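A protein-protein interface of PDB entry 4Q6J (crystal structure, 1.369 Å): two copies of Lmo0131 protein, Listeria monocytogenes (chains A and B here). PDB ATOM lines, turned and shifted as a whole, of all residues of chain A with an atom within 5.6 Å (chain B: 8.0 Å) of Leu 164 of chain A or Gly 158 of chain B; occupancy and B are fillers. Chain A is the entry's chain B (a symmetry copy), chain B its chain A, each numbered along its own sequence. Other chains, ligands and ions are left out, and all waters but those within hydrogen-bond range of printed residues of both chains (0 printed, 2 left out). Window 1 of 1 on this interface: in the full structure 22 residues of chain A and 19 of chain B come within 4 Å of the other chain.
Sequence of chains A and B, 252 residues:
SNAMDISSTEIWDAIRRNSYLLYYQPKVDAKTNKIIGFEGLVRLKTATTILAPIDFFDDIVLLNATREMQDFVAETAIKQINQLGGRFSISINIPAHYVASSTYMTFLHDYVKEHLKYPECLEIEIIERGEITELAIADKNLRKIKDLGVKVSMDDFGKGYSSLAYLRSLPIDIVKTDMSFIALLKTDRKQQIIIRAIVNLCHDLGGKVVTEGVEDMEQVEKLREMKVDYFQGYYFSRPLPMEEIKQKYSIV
The backbone carbonyl oxygen (O) of Gly 160 of chain B is in hydrogen-bond range of the backbone NH (N) of Ser 162 of chain A.
The side-chain amino group (NZ) of Lys 190 of chain B lies within hydrogen-bond range of the backbone carbonyl oxygen (O) of Leu 167 of chain A (3.0 Å).
O of Arg 168 of chain A sits at hydrogen-bond distance from NZ of Lys 190 of chain B, 3.2 Å away.
OG of Ser 163 of chain B sits at hydrogen-bond distance from N of Gly 158 of chain B.
The backbone carbonyl oxygen (O) of Phe 181 of chain B lies within hydrogen-bond range of the side-chain amide nitrogen (NE2) of Gln 191 of chain B (2.9 Å).
CD1 of Leu 164 of chain B touches CE1 of Phe 157 of chain A (3.7 Å).
Tyr 161 of chain A touches Gly 160 of chain B.
CD2 of Tyr 161 of chain A touches CE2 of Tyr 161 of chain B, at 3.7 Å.
Ser 162 of chain A touches Gly 158 of chain B (CA to O, 3.9 Å).
Leu 164 of chain A touches Gly 158 of chain B.
CD of Arg 168 of chain A touches OE1 of Gln 191 of chain B, 3.3 Å away.
Arg 168 of chain A touches Ile 194 of chain B.
CD1 of Leu 201 of chain A touches CA of Ile 194 of chain B, at 3.9 Å.
Ala 197 of chain B touches Leu 201 of chain A (CB to CD1, 3.7 Å).
Of the printed residues of chain B, Phe 157 of chain A touches Leu 164.
No residue of chain B comes within 4 Å of Ala 165 of chain A.
Of the printed residues of chain A, Lys 190 of chain B touches Leu 167 and Arg 168.
The nearest printed residue of chain A that does not touch Gly 158 of chain B is Ser 163 of chain A (4.6 Å).
Of the 12 printed residues of chain A, 7 touch a printed residue of chain B.
Printed residues of chain A that touch a printed residue of chain B: Phe 157, Tyr 161, Ser 162, Leu 164, Leu 167, Arg 168 and Leu 201.
Hydrophobic or aromatic side chains of chain B that line the printed part of chain A: Tyr 161, Leu 164, Ile 194 and Ala 197.
Phe 157 of chain A touches Leu 164 of chain B, but with the chains exchanged Leu 164 of chain A does not touch Phe 157 of chain B (4.1 Å).
Tyr 161 of chain A touches its own counterpart, Tyr 161 of chain B.
Positions printed for both chains: 154, 157, 161, 162, 163, 164 and 201.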
ATOM      1  N   MET A 154     -20.757  28.124  -6.739  1.00  0.00           N
ATOM      2  CA  MET A 154     -20.105  26.937  -6.188  1.00  0.00           C
ATOM      3  C   MET A 154     -18.869  26.671  -7.011  1.00  0.00           C
ATOM      4  O   MET A 154     -18.877  26.821  -8.227  1.00  0.00           O
ATOM      5  CB  MET A 154     -21.056  25.721  -6.195  1.00  0.00           C
ATOM      6  CG  MET A 154     -21.497  25.285  -7.563  1.00  0.00           C
ATOM      7  SD  MET A 154     -22.723  23.743  -7.617  1.00  0.00           S
ATOM      8  CE  MET A 154     -21.409  22.358  -7.056  1.00  0.00           C
ATOM      9  N   PHE A 157     -16.736  22.640 -10.045  1.00  0.00           N
ATOM     10  CA  PHE A 157     -17.877  21.861 -10.458  1.00  0.00           C
ATOM     11  C   PHE A 157     -17.428  20.576 -11.126  1.00  0.00           C
ATOM     12  O   PHE A 157     -16.770  20.549 -12.136  1.00  0.00           O
ATOM     13  CB  PHE A 157     -18.858  22.615 -11.378  1.00  0.00           C
ATOM     14  CG  PHE A 157     -20.100  21.815 -11.681  1.00  0.00           C
ATOM     15  CD1 PHE A 157     -20.109  20.919 -12.724  1.00  0.00           C
ATOM     16  CD2 PHE A 157     -21.201  21.877 -10.863  1.00  0.00           C
ATOM     17  CE1 PHE A 157     -21.216  20.159 -12.989  1.00  0.00           C
ATOM     18  CE2 PHE A 157     -22.312  21.101 -11.119  1.00  0.00           C
ATOM     19  CZ  PHE A 157     -22.321  20.247 -12.185  1.00  0.00           C
ATOM     20  N   TYR A 161     -17.026  17.281  -4.454  1.00  0.00           N
ATOM     21  CA  TYR A 161     -17.966  16.296  -4.049  1.00  0.00           C
ATOM     22  C   TYR A 161     -19.359  16.594  -4.567  1.00  0.00           C
ATOM     23  O   TYR A 161     -19.861  17.691  -4.440  1.00  0.00           O
ATOM     24  CB  TYR A 161     -17.982  16.272  -2.550  1.00  0.00           C
ATOM     25  CG  TYR A 161     -18.755  15.147  -1.970  1.00  0.00           C
ATOM     26  CD1 TYR A 161     -19.936  15.374  -1.290  1.00  0.00           C
ATOM     27  CD2 TYR A 161     -18.311  13.854  -2.100  1.00  0.00           C
ATOM     28  CE1 TYR A 161     -20.657  14.331  -0.756  1.00  0.00           C
ATOM     29  CE2 TYR A 161     -19.013  12.814  -1.557  1.00  0.00           C
ATOM     30  CZ  TYR A 161     -20.180  13.058  -0.890  1.00  0.00           C
ATOM     31  OH  TYR A 161     -20.862  12.003  -0.368  1.00  0.00           O
ATOM     32  N   SER A 162     -19.993  15.594  -5.143  1.00  0.00           N
ATOM     33  CA  SER A 162     -21.434  15.596  -5.365  1.00  0.00           C
ATOM     34  C   SER A 162     -21.904  16.934  -5.926  1.00  0.00           C
ATOM     35  O   SER A 162     -22.801  17.569  -5.371  1.00  0.00           O
ATOM     36  CB  SER A 162     -22.175  15.281  -4.064  1.00  0.00           C
ATOM     37  OG  SER A 162     -22.380  13.886  -3.919  1.00  0.00           O
ATOM     38  N   SER A 163     -21.294  17.355  -7.028  1.00  0.00           N
ATOM     39  CA  SER A 163     -21.595  18.645  -7.622  1.00  0.00           C
ATOM     40  C   SER A 163     -23.032  18.698  -8.115  1.00  0.00           C
ATOM     41  O   SER A 163     -23.664  19.731  -8.091  1.00  0.00           O
ATOM     42  CB  SER A 163     -20.621  18.929  -8.768  1.00  0.00           C
ATOM     43  OG  SER A 163     -19.300  18.892  -8.297  1.00  0.00           O
ATOM     44  N   LEU A 164     -23.516  17.591  -8.634  1.00  0.00           N
ATOM     45  CA  LEU A 164     -24.884  17.544  -9.125  1.00  0.00           C
ATOM     46  C   LEU A 164     -25.938  17.734  -8.045  1.00  0.00           C
ATOM     47  O   LEU A 164     -26.974  18.309  -8.300  1.00  0.00           O
ATOM     48  CB  LEU A 164     -25.147  16.284  -9.943  1.00  0.00           C
ATOM     49  CG  LEU A 164     -24.688  16.447 -11.382  1.00  0.00           C
ATOM     50  CD1 LEU A 164     -25.062  15.210 -12.176  1.00  0.00           C
ATOM     51  CD2 LEU A 164     -25.266  17.676 -12.046  1.00  0.00           C
ATOM     52  N   ALA A 165     -25.669  17.203  -6.854  1.00  0.00           N
ATOM     53  CA  ALA A 165     -26.580  17.335  -5.719  1.00  0.00           C
ATOM     54  C   ALA A 165     -26.574  18.752  -5.161  1.00  0.00           C
ATOM     55  O   ALA A 165     -27.607  19.278  -4.780  1.00  0.00           O
ATOM     56  CB  ALA A 165     -26.231  16.376  -4.658  1.00  0.00           C
ATOM     57  N   TYR A 166     -25.399  19.361  -5.104  1.00  0.00           N
ATOM     58  CA  TYR A 166     -25.314  20.779  -4.806  1.00  0.00           C
ATOM     59  C   TYR A 166     -26.175  21.591  -5.757  1.00  0.00           C
ATOM     60  O   TYR A 166     -26.957  22.456  -5.360  1.00  0.00           O
ATOM     61  CB  TYR A 166     -23.871  21.248  -4.904  1.00  0.00           C
ATOM     62  CG  TYR A 166     -23.111  21.008  -3.641  1.00  0.00           C
ATOM     63  CD1 TYR A 166     -22.507  19.790  -3.387  1.00  0.00           C
ATOM     64  CD2 TYR A 166     -22.998  21.995  -2.687  1.00  0.00           C
ATOM     65  CE1 TYR A 166     -21.795  19.578  -2.200  1.00  0.00           C
ATOM     66  CE2 TYR A 166     -22.306  21.790  -1.499  1.00  0.00           C
ATOM     67  CZ  TYR A 166     -21.707  20.590  -1.250  1.00  0.00           C
ATOM     68  OH  TYR A 166     -21.005  20.407  -0.065  1.00  0.00           O
ATOM     69  N   LEU A 167     -26.023  21.298  -7.032  1.00  0.00           N
ATOM     70  CA  LEU A 167     -26.769  21.986  -8.058  1.00  0.00           C
ATOM     71  C   LEU A 167     -28.265  21.803  -7.907  1.00  0.00           C
ATOM     72  O   LEU A 167     -29.026  22.735  -8.089  1.00  0.00           O
ATOM     73  CB  LEU A 167     -26.326  21.473  -9.426  1.00  0.00           C
ATOM     74  CG  LEU A 167     -26.760  22.349 -10.578  1.00  0.00           C
ATOM     75  CD1 LEU A 167     -26.469  23.807 -10.319  1.00  0.00           C
ATOM     76  CD2 LEU A 167     -26.005  21.894 -11.771  1.00  0.00           C
ATOM     77  N   ARG A 168     -28.673  20.580  -7.579  1.00  0.00           N
ATOM     78  CA  ARG A 168     -30.066  20.230  -7.398  1.00  0.00           C
ATOM     79  C   ARG A 168     -30.685  20.900  -6.176  1.00  0.00           C
ATOM     80  O   ARG A 168     -31.753  21.481  -6.271  1.00  0.00           O
ATOM     81  CB  ARG A 168     -30.184  18.719  -7.250  1.00  0.00           C
ATOM     82  CG  ARG A 168     -31.523  18.269  -6.773  1.00  0.00           C
ATOM     83  CD  ARG A 168     -31.549  16.792  -6.460  1.00  0.00           C
ATOM     84  NE  ARG A 168     -32.929  16.326  -6.361  1.00  0.00           N
ATOM     85  CZ  ARG A 168     -33.305  15.054  -6.354  1.00  0.00           C
ATOM     86  NH1 ARG A 168     -32.420  14.078  -6.439  1.00  0.00           N
ATOM     87  NH2 ARG A 168     -34.578  14.777  -6.270  1.00  0.00           N
ATOM     88  N   SER A 169     -29.997  20.851  -5.038  1.00  0.00           N
ATOM     89  CA  SER A 169     -30.629  21.187  -3.775  1.00  0.00           C
ATOM     90  C   SER A 169     -30.173  22.474  -3.061  1.00  0.00           C
ATOM     91  O   SER A 169     -30.621  22.752  -1.944  1.00  0.00           O
ATOM     92  CB  SER A 169     -30.550  19.988  -2.841  1.00  0.00           C
ATOM     93  OG  SER A 169     -30.990  18.823  -3.515  1.00  0.00           O
ATOM     94  N   LEU A 201     -27.128  23.323 -19.382  1.00  0.00           N
ATOM     95  CA  LEU A 201     -27.843  22.925 -18.185  1.00  0.00           C
ATOM     96  C   LEU A 201     -27.942  24.111 -17.211  1.00  0.00           C
ATOM     97  O   LEU A 201     -29.015  24.433 -16.711  1.00  0.00           O
ATOM     98  CB  LEU A 201     -27.152  21.745 -17.531  1.00  0.00           C
ATOM     99  CG  LEU A 201     -27.716  21.341 -16.152  1.00  0.00           C
ATOM    100  CD1 LEU A 201     -29.238  21.035 -16.168  1.00  0.00           C
ATOM    101  CD2 LEU A 201     -26.899  20.189 -15.573  1.00  0.00           C
ATOM    102  N   ARG B 129     -15.868   4.550  -6.830  1.00  0.00           N
ATOM    103  CA  ARG B 129     -15.061   5.457  -7.608  1.00  0.00           C
ATOM    104  C   ARG B 129     -14.464   6.600  -6.772  1.00  0.00           C
ATOM    105  O   ARG B 129     -13.279   6.589  -6.429  1.00  0.00           O
ATOM    106  CB  ARG B 129     -15.940   5.970  -8.753  1.00  0.00           C
ATOM    107  CG  ARG B 129     -15.796   7.413  -9.138  1.00  0.00           C
ATOM    108  CD  ARG B 129     -16.692   7.717 -10.328  1.00  0.00           C
ATOM    109  NE  ARG B 129     -18.060   7.955  -9.906  1.00  0.00           N
ATOM    110  CZ  ARG B 129     -19.051   7.077 -10.009  1.00  0.00           C
ATOM    111  NH1 ARG B 129     -18.851   5.868 -10.536  1.00  0.00           N
ATOM    112  NH2 ARG B 129     -20.250   7.413  -9.568  1.00  0.00           N
ATOM    113  N   MET B 154     -20.784   2.686 -15.426  1.00  0.00           N
ATOM    114  CA  MET B 154     -20.393   3.244 -14.146  1.00  0.00           C
ATOM    115  C   MET B 154     -21.637   3.494 -13.346  1.00  0.00           C
ATOM    116  O   MET B 154     -22.628   3.992 -13.871  1.00  0.00           O
ATOM    117  CB  MET B 154     -19.601   4.547 -14.333  1.00  0.00           C
ATOM    118  CG  MET B 154     -20.326   5.597 -15.157  1.00  0.00           C
ATOM    119  SD  MET B 154     -19.345   7.247 -15.365  1.00  0.00           S
ATOM    120  CE  MET B 154     -19.373   7.787 -13.454  1.00  0.00           C
ATOM    121  N   ASP B 155     -21.596   3.158 -12.070  1.00  0.00           N
ATOM    122  CA  ASP B 155     -22.806   3.320 -11.295  1.00  0.00           C
ATOM    123  C   ASP B 155     -22.866   4.615 -10.530  1.00  0.00           C
ATOM    124  O   ASP B 155     -21.885   5.356 -10.460  1.00  0.00           O
ATOM    125  CB  ASP B 155     -23.075   2.117 -10.396  1.00  0.00           C
ATOM    126  CG  ASP B 155     -22.198   2.077  -9.180  1.00  0.00           C
ATOM    127  OD1 ASP B 155     -21.158   2.754  -9.175  1.00  0.00           O
ATOM    128  OD2 ASP B 155     -22.550   1.360  -8.219  1.00  0.00           O
ATOM    129  N   ASP B 156     -24.031   4.889  -9.978  1.00  0.00           N
ATOM    130  CA  ASP B 156     -24.254   6.035  -9.102  1.00  0.00           C
ATOM    131  C   ASP B 156     -23.696   7.325  -9.670  1.00  0.00           C
ATOM    132  O   ASP B 156     -23.026   8.078  -8.989  1.00  0.00           O
ATOM    133  CB  ASP B 156     -23.675   5.783  -7.701  1.00  0.00           C
ATOM    134  CG  ASP B 156     -24.358   4.633  -6.973  1.00  0.00           C
ATOM    135  OD1 ASP B 156     -25.469   4.224  -7.363  1.00  0.00           O
ATOM    136  OD2 ASP B 156     -23.778   4.135  -5.994  1.00  0.00           O
ATOM    137  N   PHE B 157     -23.949   7.563 -10.938  1.00  0.00           N
ATOM    138  CA  PHE B 157     -23.521   8.798 -11.533  1.00  0.00           C
ATOM    139  C   PHE B 157     -24.186   9.958 -10.793  1.00  0.00           C
ATOM    140  O   PHE B 157     -25.339   9.884 -10.413  1.00  0.00           O
ATOM    141  CB  PHE B 157     -23.916   8.811 -12.993  1.00  0.00           C
ATOM    142  CG  PHE B 157     -23.367   9.976 -13.749  1.00  0.00           C
ATOM    143  CD1 PHE B 157     -24.057  11.176 -13.808  1.00  0.00           C
ATOM    144  CD2 PHE B 157     -22.153   9.886 -14.383  1.00  0.00           C
ATOM    145  CE1 PHE B 157     -23.536  12.250 -14.489  1.00  0.00           C
ATOM    146  CE2 PHE B 157     -21.633  10.964 -15.073  1.00  0.00           C
ATOM    147  CZ  PHE B 157     -22.325  12.138 -15.126  1.00  0.00           C
ATOM    148  N   GLY B 158     -23.445  11.033 -10.578  1.00  0.00           N
ATOM    149  CA  GLY B 158     -23.975  12.164  -9.839  1.00  0.00           C
ATOM    150  C   GLY B 158     -23.495  12.148  -8.404  1.00  0.00           C
ATOM    151  O   GLY B 158     -23.162  13.199  -7.835  1.00  0.00           O
ATOM    152  N   LYS B 159     -23.378  10.950  -7.834  1.00  0.00           N
ATOM    153  CA  LYS B 159     -22.960  10.707  -6.449  1.00  0.00           C
ATOM    154  C   LYS B 159     -21.440  10.594  -6.266  1.00  0.00           C
ATOM    155  O   LYS B 159     -20.769   9.829  -6.936  1.00  0.00           O
ATOM    156  CB  LYS B 159     -23.655   9.433  -5.931  1.00  0.00           C
ATOM    157  CG  LYS B 159     -24.012   9.420  -4.458  1.00  0.00           C
ATOM    158  CD  LYS B 159     -24.042   8.005  -3.906  1.00  0.00           C
ATOM    159  CE  LYS B 159     -25.351   7.312  -4.217  1.00  0.00           C
ATOM    160  NZ  LYS B 159     -25.421   5.917  -3.698  1.00  0.00           N
ATOM    161  N   GLY B 160     -20.902  11.337  -5.296  1.00  0.00           N
ATOM    162  CA  GLY B 160     -19.496  11.218  -4.954  1.00  0.00           C
ATOM    163  C   GLY B 160     -18.515  11.987  -5.810  1.00  0.00           C
ATOM    164  O   GLY B 160     -18.842  13.017  -6.346  1.00  0.00           O
ATOM    165  N   TYR B 161     -17.286  11.510  -5.889  1.00  0.00           N
ATOM    166  CA  TYR B 161     -16.246  12.217  -6.628  1.00  0.00           C
ATOM    167  C   TYR B 161     -16.123  11.917  -8.145  1.00  0.00           C
ATOM    168  O   TYR B 161     -16.209  10.779  -8.599  1.00  0.00           O
ATOM    169  CB  TYR B 161     -14.884  12.062  -5.939  1.00  0.00           C
ATOM    170  CG  TYR B 161     -14.655  12.966  -4.753  1.00  0.00           C
ATOM    171  CD1 TYR B 161     -14.226  14.272  -4.917  1.00  0.00           C
ATOM    172  CD2 TYR B 161     -14.862  12.511  -3.475  1.00  0.00           C
ATOM    173  CE1 TYR B 161     -14.013  15.093  -3.834  1.00  0.00           C
ATOM    174  CE2 TYR B 161     -14.655  13.327  -2.388  1.00  0.00           C
ATOM    175  CZ  TYR B 161     -14.226  14.614  -2.575  1.00  0.00           C
ATOM    176  OH  TYR B 161     -14.010  15.414  -1.488  1.00  0.00           O
ATOM    177  N   SER B 162     -15.970  13.001  -8.886  1.00  0.00           N
ATOM    178  CA  SER B 162     -15.479  13.029 -10.249  1.00  0.00           C
ATOM    179  C   SER B 162     -16.255  12.275 -11.342  1.00  0.00           C
ATOM    180  O   SER B 162     -15.668  11.741 -12.245  1.00  0.00           O
ATOM    181  CB  SER B 162     -14.036  12.539 -10.243  1.00  0.00           C
ATOM    182  OG  SER B 162     -13.355  13.069  -9.141  1.00  0.00           O
ATOM    183  N   SER B 163     -17.570  12.268 -11.256  1.00  0.00           N
ATOM    184  CA  SER B 163     -18.414  11.526 -12.155  1.00  0.00           C
ATOM    185  C   SER B 163     -18.118  11.970 -13.586  1.00  0.00           C
ATOM    186  O   SER B 163     -17.823  11.146 -14.451  1.00  0.00           O
ATOM    187  CB  SER B 163     -19.889  11.704 -11.778  1.00  0.00           C
ATOM    188  OG  SER B 163     -20.192  11.000 -10.589  1.00  0.00           O
ATOM    189  N   LEU B 164     -18.132  13.281 -13.805  1.00  0.00           N
ATOM    190  CA  LEU B 164     -17.842  13.842 -15.108  1.00  0.00           C
ATOM    191  C   LEU B 164     -16.394  13.563 -15.527  1.00  0.00           C
ATOM    192  O   LEU B 164     -16.112  13.441 -16.712  1.00  0.00           O
ATOM    193  CB  LEU B 164     -18.105  15.339 -15.096  1.00  0.00           C
ATOM    194  CG  LEU B 164     -19.576  15.696 -14.960  1.00  0.00           C
ATOM    195  CD1 LEU B 164     -19.763  17.167 -14.695  1.00  0.00           C
ATOM    196  CD2 LEU B 164     -20.356  15.287 -16.188  1.00  0.00           C
ATOM    197  N   VAL B 175     -24.086   4.812 -18.321  1.00  0.00           N
ATOM    198  CA  VAL B 175     -24.041   5.500 -17.035  1.00  0.00           C
ATOM    199  C   VAL B 175     -25.238   5.021 -16.237  1.00  0.00           C
ATOM    200  O   VAL B 175     -26.343   4.968 -16.779  1.00  0.00           O
ATOM    201  CB  VAL B 175     -24.083   7.021 -17.236  1.00  0.00           C
ATOM    202  CG1 VAL B 175     -24.793   7.711 -16.112  1.00  0.00           C
ATOM    203  CG2 VAL B 175     -22.678   7.582 -17.438  1.00  0.00           C
ATOM    204  N   LYS B 176     -25.011   4.623 -14.990  1.00  0.00           N
ATOM    205  CA  LYS B 176     -26.090   4.240 -14.100  1.00  0.00           C
ATOM    206  C   LYS B 176     -26.261   5.318 -13.033  1.00  0.00           C
ATOM    207  O   LYS B 176     -25.270   5.839 -12.497  1.00  0.00           O
ATOM    208  CB  LYS B 176     -25.838   2.887 -13.429  1.00  0.00           C
ATOM    209  CG  LYS B 176     -25.391   1.813 -14.372  1.00  0.00           C
ATOM    210  CD  LYS B 176     -25.395   0.456 -13.696  1.00  0.00           C
ATOM    211  CE  LYS B 176     -26.770  -0.150 -13.667  1.00  0.00           C
ATOM    212  NZ  LYS B 176     -26.919  -1.344 -12.783  1.00  0.00           N
ATOM    213  N   THR B 177     -27.511   5.651 -12.729  1.00  0.00           N
ATOM    214  CA  THR B 177     -27.801   6.571 -11.635  1.00  0.00           C
ATOM    215  C   THR B 177     -28.408   5.852 -10.439  1.00  0.00           C
ATOM    216  O   THR B 177     -28.915   4.752 -10.574  1.00  0.00           O
ATOM    217  CB  THR B 177     -28.698   7.736 -12.094  1.00  0.00           C
ATOM    218  OG1 THR B 177     -29.920   7.237 -12.643  1.00  0.00           O
ATOM    219  CG2 THR B 177     -27.985   8.501 -13.142  1.00  0.00           C
ATOM    220  N   ASP B 178     -28.343   6.443  -9.252  1.00  0.00           N
ATOM    221  CA  ASP B 178     -28.949   5.757  -8.114  1.00  0.00           C
ATOM    222  C   ASP B 178     -30.404   6.168  -7.866  1.00  0.00           C
ATOM    223  O   ASP B 178     -30.956   7.069  -8.510  1.00  0.00           O
ATOM    224  CB  ASP B 178     -28.107   5.886  -6.840  1.00  0.00           C
ATOM    225  CG  ASP B 178     -28.482   7.078  -6.010  1.00  0.00           C
ATOM    226  OD1 ASP B 178     -28.671   6.929  -4.776  1.00  0.00           O
ATOM    227  OD2 ASP B 178     -28.590   8.161  -6.604  1.00  0.00           O
ATOM    228  N   PHE B 181     -31.389   9.876  -7.540  1.00  0.00           N
ATOM    229  CA  PHE B 181     -31.320  10.735  -8.696  1.00  0.00           C
ATOM    230  C   PHE B 181     -32.694  10.893  -9.306  1.00  0.00           C
ATOM    231  O   PHE B 181     -32.951  11.855 -10.028  1.00  0.00           O
ATOM    232  CB  PHE B 181     -30.411  10.109  -9.726  1.00  0.00           C
ATOM    233  CG  PHE B 181     -29.717  11.101 -10.589  1.00  0.00           C
ATOM    234  CD1 PHE B 181     -28.731  11.927 -10.066  1.00  0.00           C
ATOM    235  CD2 PHE B 181     -30.034  11.209 -11.914  1.00  0.00           C
ATOM    236  CE1 PHE B 181     -28.095  12.833 -10.850  1.00  0.00           C
ATOM    237  CE2 PHE B 181     -29.369  12.129 -12.718  1.00  0.00           C
ATOM    238  CZ  PHE B 181     -28.404  12.938 -12.177  1.00  0.00           C
ATOM    239  N   LYS B 190     -35.988  21.340 -10.960  1.00  0.00           N
ATOM    240  CA  LYS B 190     -34.552  21.339 -11.161  1.00  0.00           C
ATOM    241  C   LYS B 190     -33.994  19.923 -11.441  1.00  0.00           C
ATOM    242  O   LYS B 190     -33.217  19.738 -12.357  1.00  0.00           O
ATOM    243  CB  LYS B 190     -33.846  21.993  -9.965  1.00  0.00           C
ATOM    244  CG  LYS B 190     -34.074  23.479  -9.836  1.00  0.00           C
ATOM    245  CD  LYS B 190     -33.471  24.071  -8.520  1.00  0.00           C
ATOM    246  CE  LYS B 190     -31.918  24.040  -8.433  1.00  0.00           C
ATOM    247  NZ  LYS B 190     -31.290  24.537  -7.138  1.00  0.00           N
ATOM    248  N   GLN B 191     -34.397  18.916 -10.676  1.00  0.00           N
ATOM    249  CA  GLN B 191     -33.861  17.590 -10.953  1.00  0.00           C
ATOM    250  C   GLN B 191     -34.325  17.071 -12.299  1.00  0.00           C
ATOM    251  O   GLN B 191     -33.598  16.373 -12.979  1.00  0.00           O
ATOM    252  CB  GLN B 191     -34.185  16.591  -9.843  1.00  0.00           C
ATOM    253  CG  GLN B 191     -33.464  15.217  -9.977  1.00  0.00           C
ATOM    254  CD  GLN B 191     -31.932  15.298  -9.988  1.00  0.00           C
ATOM    255  OE1 GLN B 191     -31.328  16.346  -9.693  1.00  0.00           O
ATOM    256  NE2 GLN B 191     -31.296  14.176 -10.323  1.00  0.00           N
ATOM    257  N   ILE B 194     -32.056  18.489 -14.749  1.00  0.00           N
ATOM    258  CA  ILE B 194     -30.784  17.796 -14.610  1.00  0.00           C
ATOM    259  C   ILE B 194     -30.779  16.404 -15.232  1.00  0.00           C
ATOM    260  O   ILE B 194     -29.859  16.028 -15.948  1.00  0.00           O
ATOM    261  CB  ILE B 194     -30.390  17.710 -13.141  1.00  0.00           C
ATOM    262  CG1 ILE B 194     -30.004  19.118 -12.654  1.00  0.00           C
ATOM    263  CG2 ILE B 194     -29.256  16.713 -12.943  1.00  0.00           C
ATOM    264  CD1 ILE B 194     -29.816  19.291 -11.179  1.00  0.00           C
ATOM    265  N   ILE B 195     -31.819  15.639 -14.949  1.00  0.00           N
ATOM    266  CA  ILE B 195     -31.922  14.326 -15.540  1.00  0.00           C
ATOM    267  C   ILE B 195     -31.894  14.358 -17.068  1.00  0.00           C
ATOM    268  O   ILE B 195     -31.091  13.687 -17.686  1.00  0.00           O
ATOM    269  CB  ILE B 195     -33.154  13.593 -15.043  1.00  0.00           C
ATOM    270  CG1 ILE B 195     -32.989  13.296 -13.554  1.00  0.00           C
ATOM    271  CG2 ILE B 195     -33.294  12.309 -15.804  1.00  0.00           C
ATOM    272  CD1 ILE B 195     -34.265  12.834 -12.895  1.00  0.00           C
ATOM    273  N   ALA B 197     -30.763  16.599 -18.966  1.00  0.00           N
ATOM    274  CA  ALA B 197     -29.464  17.111 -19.424  1.00  0.00           C
ATOM    275  C   ALA B 197     -28.422  15.986 -19.446  1.00  0.00           C
ATOM    276  O   ALA B 197     -27.616  15.858 -20.364  1.00  0.00           O
ATOM    277  CB  ALA B 197     -29.011  18.261 -18.548  1.00  0.00           C
ATOM    278  N   ILE B 198     -28.477  15.143 -18.438  1.00  0.00           N
ATOM    279  CA  ILE B 198     -27.541  14.056 -18.328  1.00  0.00           C
ATOM    280  C   ILE B 198     -27.859  12.976 -19.352  1.00  0.00           C
ATOM    281  O   ILE B 198     -26.974  12.463 -19.993  1.00  0.00           O
ATOM    282  CB  ILE B 198     -27.559  13.507 -16.893  1.00  0.00           C
ATOM    283  CG1 ILE B 198     -27.082  14.596 -15.921  1.00  0.00           C
ATOM    284  CG2 ILE B 198     -26.752  12.219 -16.771  1.00  0.00           C
ATOM    285  CD1 ILE B 198     -25.686  15.152 -16.224  1.00  0.00           C
ATOM    286  N   LEU B 201     -26.640  14.298 -22.523  1.00  0.00           N
ATOM    287  CA  LEU B 201     -25.188  14.213 -22.514  1.00  0.00           C
ATOM    288  C   LEU B 201     -24.699  12.805 -22.856  1.00  0.00           C
ATOM    289  O   LEU B 201     -23.867  12.631 -23.736  1.00  0.00           O
ATOM    290  CB  LEU B 201     -24.628  14.633 -21.155  1.00  0.00           C
ATOM    291  CG  LEU B 201     -23.112  14.487 -20.978  1.00  0.00           C
ATOM    292  CD1 LEU B 201     -22.287  15.142 -22.129  1.00  0.00           C
ATOM    293  CD2 LEU B 201     -22.736  15.047 -19.623  1.00  0.00           C
